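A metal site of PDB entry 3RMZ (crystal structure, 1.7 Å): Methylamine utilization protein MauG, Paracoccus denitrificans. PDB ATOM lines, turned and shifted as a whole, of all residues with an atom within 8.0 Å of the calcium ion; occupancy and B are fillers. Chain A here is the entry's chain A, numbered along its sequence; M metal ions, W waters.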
ATOM      1  N   ARG A  39      36.441 -15.198 -25.702  1.00  0.00           N
ATOM      2  CA  ARG A  39      35.557 -16.193 -24.988  1.00  0.00           C
ATOM      3  C   ARG A  39      35.464 -17.464 -25.839  1.00  0.00           C
ATOM      4  O   ARG A  39      34.369 -18.010 -26.028  1.00  0.00           O
ATOM      5  CB  ARG A  39      34.176 -15.623 -24.701  1.00  0.00           C
ATOM      6  CG  ARG A  39      33.383 -16.434 -23.569  1.00  0.00           C
ATOM      7  CD  ARG A  39      31.966 -15.902 -23.488  1.00  0.00           C
ATOM      8  NE  ARG A  39      31.306 -16.353 -22.285  1.00  0.00           N
ATOM      9  CZ  ARG A  39      30.505 -17.427 -22.238  1.00  0.00           C
ATOM     10  NH1 ARG A  39      30.370 -18.147 -23.320  1.00  0.00           N
ATOM     11  NH2 ARG A  39      29.932 -17.788 -21.071  1.00  0.00           N
ATOM     12  N   THR A  42      32.733 -17.367 -28.649  1.00  0.00           N
ATOM     13  CA  THR A  42      31.291 -17.512 -28.289  1.00  0.00           C
ATOM     14  C   THR A  42      30.853 -16.128 -27.752  1.00  0.00           C
ATOM     15  O   THR A  42      31.681 -15.181 -27.749  1.00  0.00           O
ATOM     16  CB  THR A  42      31.091 -18.601 -27.175  1.00  0.00           C
ATOM     17  OG1 THR A  42      31.779 -18.197 -25.978  1.00  0.00           O
ATOM     18  CG2 THR A  42      31.589 -19.962 -27.682  1.00  0.00           C
ATOM     19  N   ASP A  43      29.601 -16.024 -27.321  1.00  0.00           N
ATOM     20  CA  ASP A  43      29.016 -14.727 -27.081  1.00  0.00           C
ATOM     21  C   ASP A  43      28.866 -14.387 -25.598  1.00  0.00           C
ATOM     22  O   ASP A  43      28.090 -15.072 -24.879  1.00  0.00           O
ATOM     23  CB  ASP A  43      27.659 -14.654 -27.782  1.00  0.00           C
ATOM     24  CG  ASP A  43      27.104 -13.210 -27.794  1.00  0.00           C
ATOM     25  OD1 ASP A  43      25.975 -13.016 -28.363  1.00  0.00           O
ATOM     26  OD2 ASP A  43      27.730 -12.292 -27.196  1.00  0.00           O
ATOM     27  N   LEU A  51      22.698 -15.809 -21.433  1.00  0.00           N
ATOM     28  CA  LEU A  51      23.653 -16.045 -22.505  1.00  0.00           C
ATOM     29  C   LEU A  51      23.181 -17.194 -23.430  1.00  0.00           C
ATOM     30  O   LEU A  51      23.946 -17.675 -24.249  1.00  0.00           O
ATOM     31  CB  LEU A  51      25.016 -16.389 -21.926  1.00  0.00           C
ATOM     32  CG  LEU A  51      25.898 -15.158 -21.577  1.00  0.00           C
ATOM     33  CD1 LEU A  51      25.274 -14.468 -20.564  1.00  0.00           C
ATOM     34  CD2 LEU A  51      27.232 -15.706 -21.002  1.00  0.00           C
ATOM     35  N   ALA A  52      21.961 -17.635 -23.265  1.00  0.00           N
ATOM     36  CA  ALA A  52      21.498 -18.775 -24.067  1.00  0.00           C
ATOM     37  C   ALA A  52      21.474 -18.491 -25.553  1.00  0.00           C
ATOM     38  O   ALA A  52      21.799 -19.411 -26.351  1.00  0.00           O
ATOM     39  CB  ALA A  52      20.082 -19.254 -23.546  1.00  0.00           C
ATOM     40  N   ASN A  66      21.923 -21.505 -29.311  1.00  0.00           N
ATOM     41  CA  ASN A  66      23.080 -20.912 -28.646  1.00  0.00           C
ATOM     42  C   ASN A  66      24.263 -20.726 -29.622  1.00  0.00           C
ATOM     43  O   ASN A  66      24.459 -21.538 -30.499  1.00  0.00           O
ATOM     44  CB  ASN A  66      23.475 -21.870 -27.504  1.00  0.00           C
ATOM     45  CG  ASN A  66      24.658 -21.396 -26.675  1.00  0.00           C
ATOM     46  OD1 ASN A  66      25.748 -22.011 -26.693  1.00  0.00           O
ATOM     47  ND2 ASN A  66      24.484 -20.294 -25.938  1.00  0.00           N
ATOM     48  N   THR A  67      24.967 -19.635 -29.467  1.00  0.00           N
ATOM     49  CA  THR A  67      26.130 -19.411 -30.390  1.00  0.00           C
ATOM     50  C   THR A  67      27.263 -20.379 -30.063  1.00  0.00           C
ATOM     51  O   THR A  67      27.825 -20.323 -28.994  1.00  0.00           O
ATOM     52  CB  THR A  67      26.611 -17.984 -30.213  1.00  0.00           C
ATOM     53  OG1 THR A  67      25.604 -17.136 -30.775  1.00  0.00           O
ATOM     54  CG2 THR A  67      27.849 -17.724 -31.112  1.00  0.00           C
ATOM     55  N   PRO A  68      27.642 -21.249 -31.008  1.00  0.00           N
ATOM     56  CA  PRO A  68      28.698 -22.229 -30.702  1.00  0.00           C
ATOM     57  C   PRO A  68      30.088 -21.610 -30.919  1.00  0.00           C
ATOM     58  O   PRO A  68      30.318 -20.641 -31.679  1.00  0.00           O
ATOM     59  CB  PRO A  68      28.407 -23.357 -31.733  1.00  0.00           C
ATOM     60  CG  PRO A  68      27.900 -22.511 -32.924  1.00  0.00           C
ATOM     61  CD  PRO A  68      27.101 -21.399 -32.353  1.00  0.00           C
ATOM     62  N   THR A  69      31.079 -22.222 -30.275  1.00  0.00           N
ATOM     63  CA  THR A  69      32.479 -21.865 -30.617  1.00  0.00           C
ATOM     64  C   THR A  69      32.811 -22.107 -32.084  1.00  0.00           C
ATOM     65  O   THR A  69      32.319 -23.043 -32.750  1.00  0.00           O
ATOM     66  CB  THR A  69      33.450 -22.683 -29.693  1.00  0.00           C
ATOM     67  OG1 THR A  69      34.763 -22.228 -29.913  1.00  0.00           O
ATOM     68  CG2 THR A  69      33.405 -24.223 -30.089  1.00  0.00           C
ATOM     69  N   TRP A  93      24.121 -26.229 -35.660  1.00  0.00           N
ATOM     70  CA  TRP A  93      23.620 -27.330 -34.824  1.00  0.00           C
ATOM     71  C   TRP A  93      22.746 -28.367 -35.565  1.00  0.00           C
ATOM     72  O   TRP A  93      22.690 -29.509 -35.110  1.00  0.00           O
ATOM     73  CB  TRP A  93      22.805 -26.800 -33.638  1.00  0.00           C
ATOM     74  CG  TRP A  93      23.574 -26.033 -32.599  1.00  0.00           C
ATOM     75  CD1 TRP A  93      23.704 -24.641 -32.435  1.00  0.00           C
ATOM     76  CD2 TRP A  93      24.200 -26.603 -31.456  1.00  0.00           C
ATOM     77  NE1 TRP A  93      24.458 -24.358 -31.288  1.00  0.00           N
ATOM     78  CE2 TRP A  93      24.754 -25.538 -30.678  1.00  0.00           C
ATOM     79  CE3 TRP A  93      24.378 -27.927 -31.021  1.00  0.00           C
ATOM     80  CZ2 TRP A  93      25.450 -25.749 -29.468  1.00  0.00           C
ATOM     81  CZ3 TRP A  93      25.105 -28.139 -29.814  1.00  0.00           C
ATOM     82  CH2 TRP A  93      25.606 -27.048 -29.051  1.00  0.00           C
ATOM     83  N   ASN A 271      37.193 -26.681 -25.217  1.00  0.00           N
ATOM     84  CA  ASN A 271      36.822 -25.393 -24.569  1.00  0.00           C
ATOM     85  C   ASN A 271      35.469 -25.404 -23.933  1.00  0.00           C
ATOM     86  O   ASN A 271      34.981 -24.365 -23.563  1.00  0.00           O
ATOM     87  CB  ASN A 271      36.885 -24.233 -25.591  1.00  0.00           C
ATOM     88  CG  ASN A 271      38.341 -23.933 -26.003  1.00  0.00           C
ATOM     89  OD1 ASN A 271      39.198 -23.901 -25.108  1.00  0.00           O
ATOM     90  ND2 ASN A 271      38.620 -23.764 -27.316  1.00  0.00           N
ATOM     91  N   VAL A 272      34.828 -26.590 -23.819  1.00  0.00           N
ATOM     92  CA  VAL A 272      33.525 -26.611 -23.195  1.00  0.00           C
ATOM     93  C   VAL A 272      33.441 -25.884 -21.845  1.00  0.00           C
ATOM     94  O   VAL A 272      32.382 -25.299 -21.534  1.00  0.00           O
ATOM     95  CB  VAL A 272      32.930 -28.095 -23.144  1.00  0.00           C
ATOM     96  CG1 VAL A 272      33.711 -28.923 -22.033  1.00  0.00           C
ATOM     97  CG2 VAL A 272      31.423 -28.067 -22.837  1.00  0.00           C
ATOM     98  N   VAL A 274      34.567 -23.185 -20.848  1.00  0.00           N
ATOM     99  CA  VAL A 274      34.510 -21.715 -20.876  1.00  0.00           C
ATOM    100  C   VAL A 274      33.476 -21.264 -21.885  1.00  0.00           C
ATOM    101  O   VAL A 274      33.334 -20.056 -22.104  1.00  0.00           O
ATOM    102  CB  VAL A 274      35.908 -21.109 -21.152  1.00  0.00           C
ATOM    103  CG1 VAL A 274      36.977 -21.576 -20.119  1.00  0.00           C
ATOM    104  CG2 VAL A 274      36.267 -21.404 -22.677  1.00  0.00           C
ATOM    105  N   THR A 275      32.655 -22.158 -22.424  1.00  0.00           N
ATOM    106  CA  THR A 275      31.633 -21.737 -23.445  1.00  0.00           C
ATOM    107  C   THR A 275      30.163 -21.983 -23.019  1.00  0.00           C
ATOM    108  O   THR A 275      29.336 -22.143 -23.895  1.00  0.00           O
ATOM    109  CB  THR A 275      31.852 -22.469 -24.762  1.00  0.00           C
ATOM    110  OG1 THR A 275      31.708 -23.891 -24.555  1.00  0.00           O
ATOM    111  CG2 THR A 275      33.258 -22.061 -25.364  1.00  0.00           C
ATOM    112  N   GLY A 276      29.878 -22.046 -21.698  1.00  0.00           N
ATOM    113  CA  GLY A 276      28.514 -22.100 -21.163  1.00  0.00           C
ATOM    114  C   GLY A 276      27.704 -20.898 -21.699  1.00  0.00           C
ATOM    115  O   GLY A 276      28.274 -19.889 -22.129  1.00  0.00           O
ATOM    116  N   PRO A 277      26.385 -21.003 -21.700  1.00  0.00           N
ATOM    117  CA  PRO A 277      25.613 -22.162 -21.268  1.00  0.00           C
ATOM    118  C   PRO A 277      25.626 -23.223 -22.397  1.00  0.00           C
ATOM    119  O   PRO A 277      26.231 -23.036 -23.487  1.00  0.00           O
ATOM    120  CB  PRO A 277      24.210 -21.574 -21.048  1.00  0.00           C
ATOM    121  CG  PRO A 277      24.130 -20.465 -22.137  1.00  0.00           C
ATOM    122  CD  PRO A 277      25.516 -19.854 -22.034  1.00  0.00           C
ATOM    123  N   TYR A 278      24.944 -24.324 -22.118  1.00  0.00           N
ATOM    124  CA  TYR A 278      25.232 -25.559 -22.894  1.00  0.00           C
ATOM    125  C   TYR A 278      24.024 -26.034 -23.626  1.00  0.00           C
ATOM    126  O   TYR A 278      22.878 -25.696 -23.280  1.00  0.00           O
ATOM    127  CB  TYR A 278      25.726 -26.609 -21.845  1.00  0.00           C
ATOM    128  CG  TYR A 278      27.002 -26.168 -21.266  1.00  0.00           C
ATOM    129  CD1 TYR A 278      27.042 -25.695 -19.936  1.00  0.00           C
ATOM    130  CD2 TYR A 278      28.170 -26.097 -22.044  1.00  0.00           C
ATOM    131  CE1 TYR A 278      28.200 -25.146 -19.425  1.00  0.00           C
ATOM    132  CE2 TYR A 278      29.365 -25.644 -21.452  1.00  0.00           C
ATOM    133  CZ  TYR A 278      29.347 -25.134 -20.204  1.00  0.00           C
ATOM    134  OH  TYR A 278      30.528 -24.698 -19.668  1.00  0.00           O
ATOM    135  N   MET A 279      24.296 -26.880 -24.613  1.00  0.00           N
ATOM    136  CA  MET A 279      23.307 -27.505 -25.513  1.00  0.00           C
ATOM    137  C   MET A 279      22.889 -26.479 -26.549  1.00  0.00           C
ATOM    138  O   MET A 279      23.243 -25.302 -26.447  1.00  0.00           O
ATOM    139  CB  MET A 279      22.086 -28.098 -24.769  1.00  0.00           C
ATOM    140  CG  MET A 279      22.506 -29.105 -23.613  1.00  0.00           C
ATOM    141  SD  MET A 279      23.489 -30.432 -24.317  1.00  0.00           S
ATOM    142  CE  MET A 279      23.952 -31.369 -22.797  1.00  0.00           C
ATOM    143  N   HIS A 280      22.145 -26.956 -27.538  1.00  0.00           N
ATOM    144  CA  HIS A 280      21.823 -26.191 -28.737  1.00  0.00           C
ATOM    145  C   HIS A 280      20.978 -24.991 -28.404  1.00  0.00           C
ATOM    146  O   HIS A 280      20.990 -24.073 -29.183  1.00  0.00           O
ATOM    147  CB  HIS A 280      21.097 -27.134 -29.721  1.00  0.00           C
ATOM    148  CG  HIS A 280      19.738 -27.575 -29.260  1.00  0.00           C
ATOM    149  ND1 HIS A 280      19.468 -28.839 -28.768  1.00  0.00           N
ATOM    150  CD2 HIS A 280      18.541 -26.906 -29.262  1.00  0.00           C
ATOM    151  CE1 HIS A 280      18.181 -28.945 -28.487  1.00  0.00           C
ATOM    152  NE2 HIS A 280      17.591 -27.782 -28.783  1.00  0.00           N
ATOM    153  N   ASN A 281      20.263 -25.032 -27.268  1.00  0.00           N
ATOM    154  CA  ASN A 281      19.423 -23.899 -26.839  1.00  0.00           C
ATOM    155  C   ASN A 281      19.955 -23.240 -25.588  1.00  0.00           C
ATOM    156  O   ASN A 281      19.265 -22.417 -24.962  1.00  0.00           O
ATOM    157  CB  ASN A 281      17.969 -24.338 -26.624  1.00  0.00           C
ATOM    158  CG  ASN A 281      17.864 -25.538 -25.692  1.00  0.00           C
ATOM    159  OD1 ASN A 281      18.845 -25.868 -24.993  1.00  0.00           O
ATOM    160  ND2 ASN A 281      16.682 -26.217 -25.651  1.00  0.00           N
ATOM    161  N   GLY A 282      21.186 -23.585 -25.178  1.00  0.00           N
ATOM    162  CA  GLY A 282      21.761 -22.847 -24.040  1.00  0.00           C
ATOM    163  C   GLY A 282      21.025 -23.111 -22.735  1.00  0.00           C
ATOM    164  O   GLY A 282      21.072 -22.300 -21.834  1.00  0.00           O
ATOM    165  N   VAL A 283      20.305 -24.222 -22.650  1.00  0.00           N
ATOM    166  CA  VAL A 283      19.350 -24.374 -21.534  1.00  0.00           C
ATOM    167  C   VAL A 283      20.033 -24.577 -20.188  1.00  0.00           C
ATOM    168  O   VAL A 283      19.468 -24.198 -19.140  1.00  0.00           O
ATOM    169  CB  VAL A 283      18.415 -25.535 -21.807  1.00  0.00           C
ATOM    170  CG1 VAL A 283      19.192 -26.872 -21.900  1.00  0.00           C
ATOM    171  CG2 VAL A 283      17.251 -25.627 -20.768  1.00  0.00           C
ATOM    172  N   PHE A 284      21.237 -25.102 -20.150  1.00  0.00           N
ATOM    173  CA  PHE A 284      21.895 -25.320 -18.840  1.00  0.00           C
ATOM    174  C   PHE A 284      23.054 -24.351 -18.690  1.00  0.00           C
ATOM    175  O   PHE A 284      23.957 -24.344 -19.511  1.00  0.00           O
ATOM    176  CB  PHE A 284      22.460 -26.760 -18.777  1.00  0.00           C
ATOM    177  CG  PHE A 284      21.442 -27.795 -19.064  1.00  0.00           C
ATOM    178  CD1 PHE A 284      20.196 -27.683 -18.446  1.00  0.00           C
ATOM    179  CD2 PHE A 284      21.754 -28.932 -19.853  1.00  0.00           C
ATOM    180  CE1 PHE A 284      19.245 -28.638 -18.659  1.00  0.00           C
ATOM    181  CE2 PHE A 284      20.751 -29.886 -20.084  1.00  0.00           C
ATOM    182  CZ  PHE A 284      19.534 -29.753 -19.474  1.00  0.00           C
HETATM  183 CA    CA M   1      27.520 -22.773 -25.395  1.00  0.00          CA
HETATM  184  O   HOH W   1      28.846 -22.144 -27.151  1.00  0.00           O
HETATM  185  O   HOH W   2      26.413 -24.727 -26.205  1.00  0.00           O
HETATM  186  O   HOH W   3      29.059 -24.566 -25.206  1.00  0.00           O
HETATM  187  O   HOH W   4      27.392 -20.295 -24.937  1.00  0.00           O
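OG1 of Thr 275 sits close to O of Asn 271.
The side-chain amide nitrogen of Asn 66 is in hydrogen-bond range of the backbone carbonyl oxygen of Ala 52 (2.9 Å).
The backbone carbonyl oxygen of Asn 66 is in hydrogen-bond range of the indole nitrogen of Trp 93, 2.9 Å away.
O of His 280 sits at hydrogen-bond distance from N of Asn 66 (2.7 Å).
ND2 of Asn 66 is in hydrogen-bond range of O of Leu 51, 3.2 Å away.
OG1 of Thr 275 is in hydrogen-bond range of O of Val 272, 3.4 Å away.
Of the 23 residues printed, 3 come within 4 Å of the calcium ion.
Water W1 is bound to the calcium ion, at 2.3 Å.
The backbone carbonyl oxygen (O) of Pro 277 binds the calcium ion (2.3 Å).
OD1 of Asn 66 is bound to the calcium ion (2.3 Å).
The calcium ion is bound by water W3, 2.4 Å away.
Water W2 is bound to the calcium ion (2.4 Å).
O of Thr 275 is bound to the calcium ion.
Water W4 is bound to the calcium ion (2.5 Å).
The calcium ion has seven donor atoms within binding distance.
Water W4 bridges the backbone carbonyl oxygen (O) of Gly 276 (3.0 Å) and the side-chain amide nitrogen (ND2) of Asn 66 (3.1 Å).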
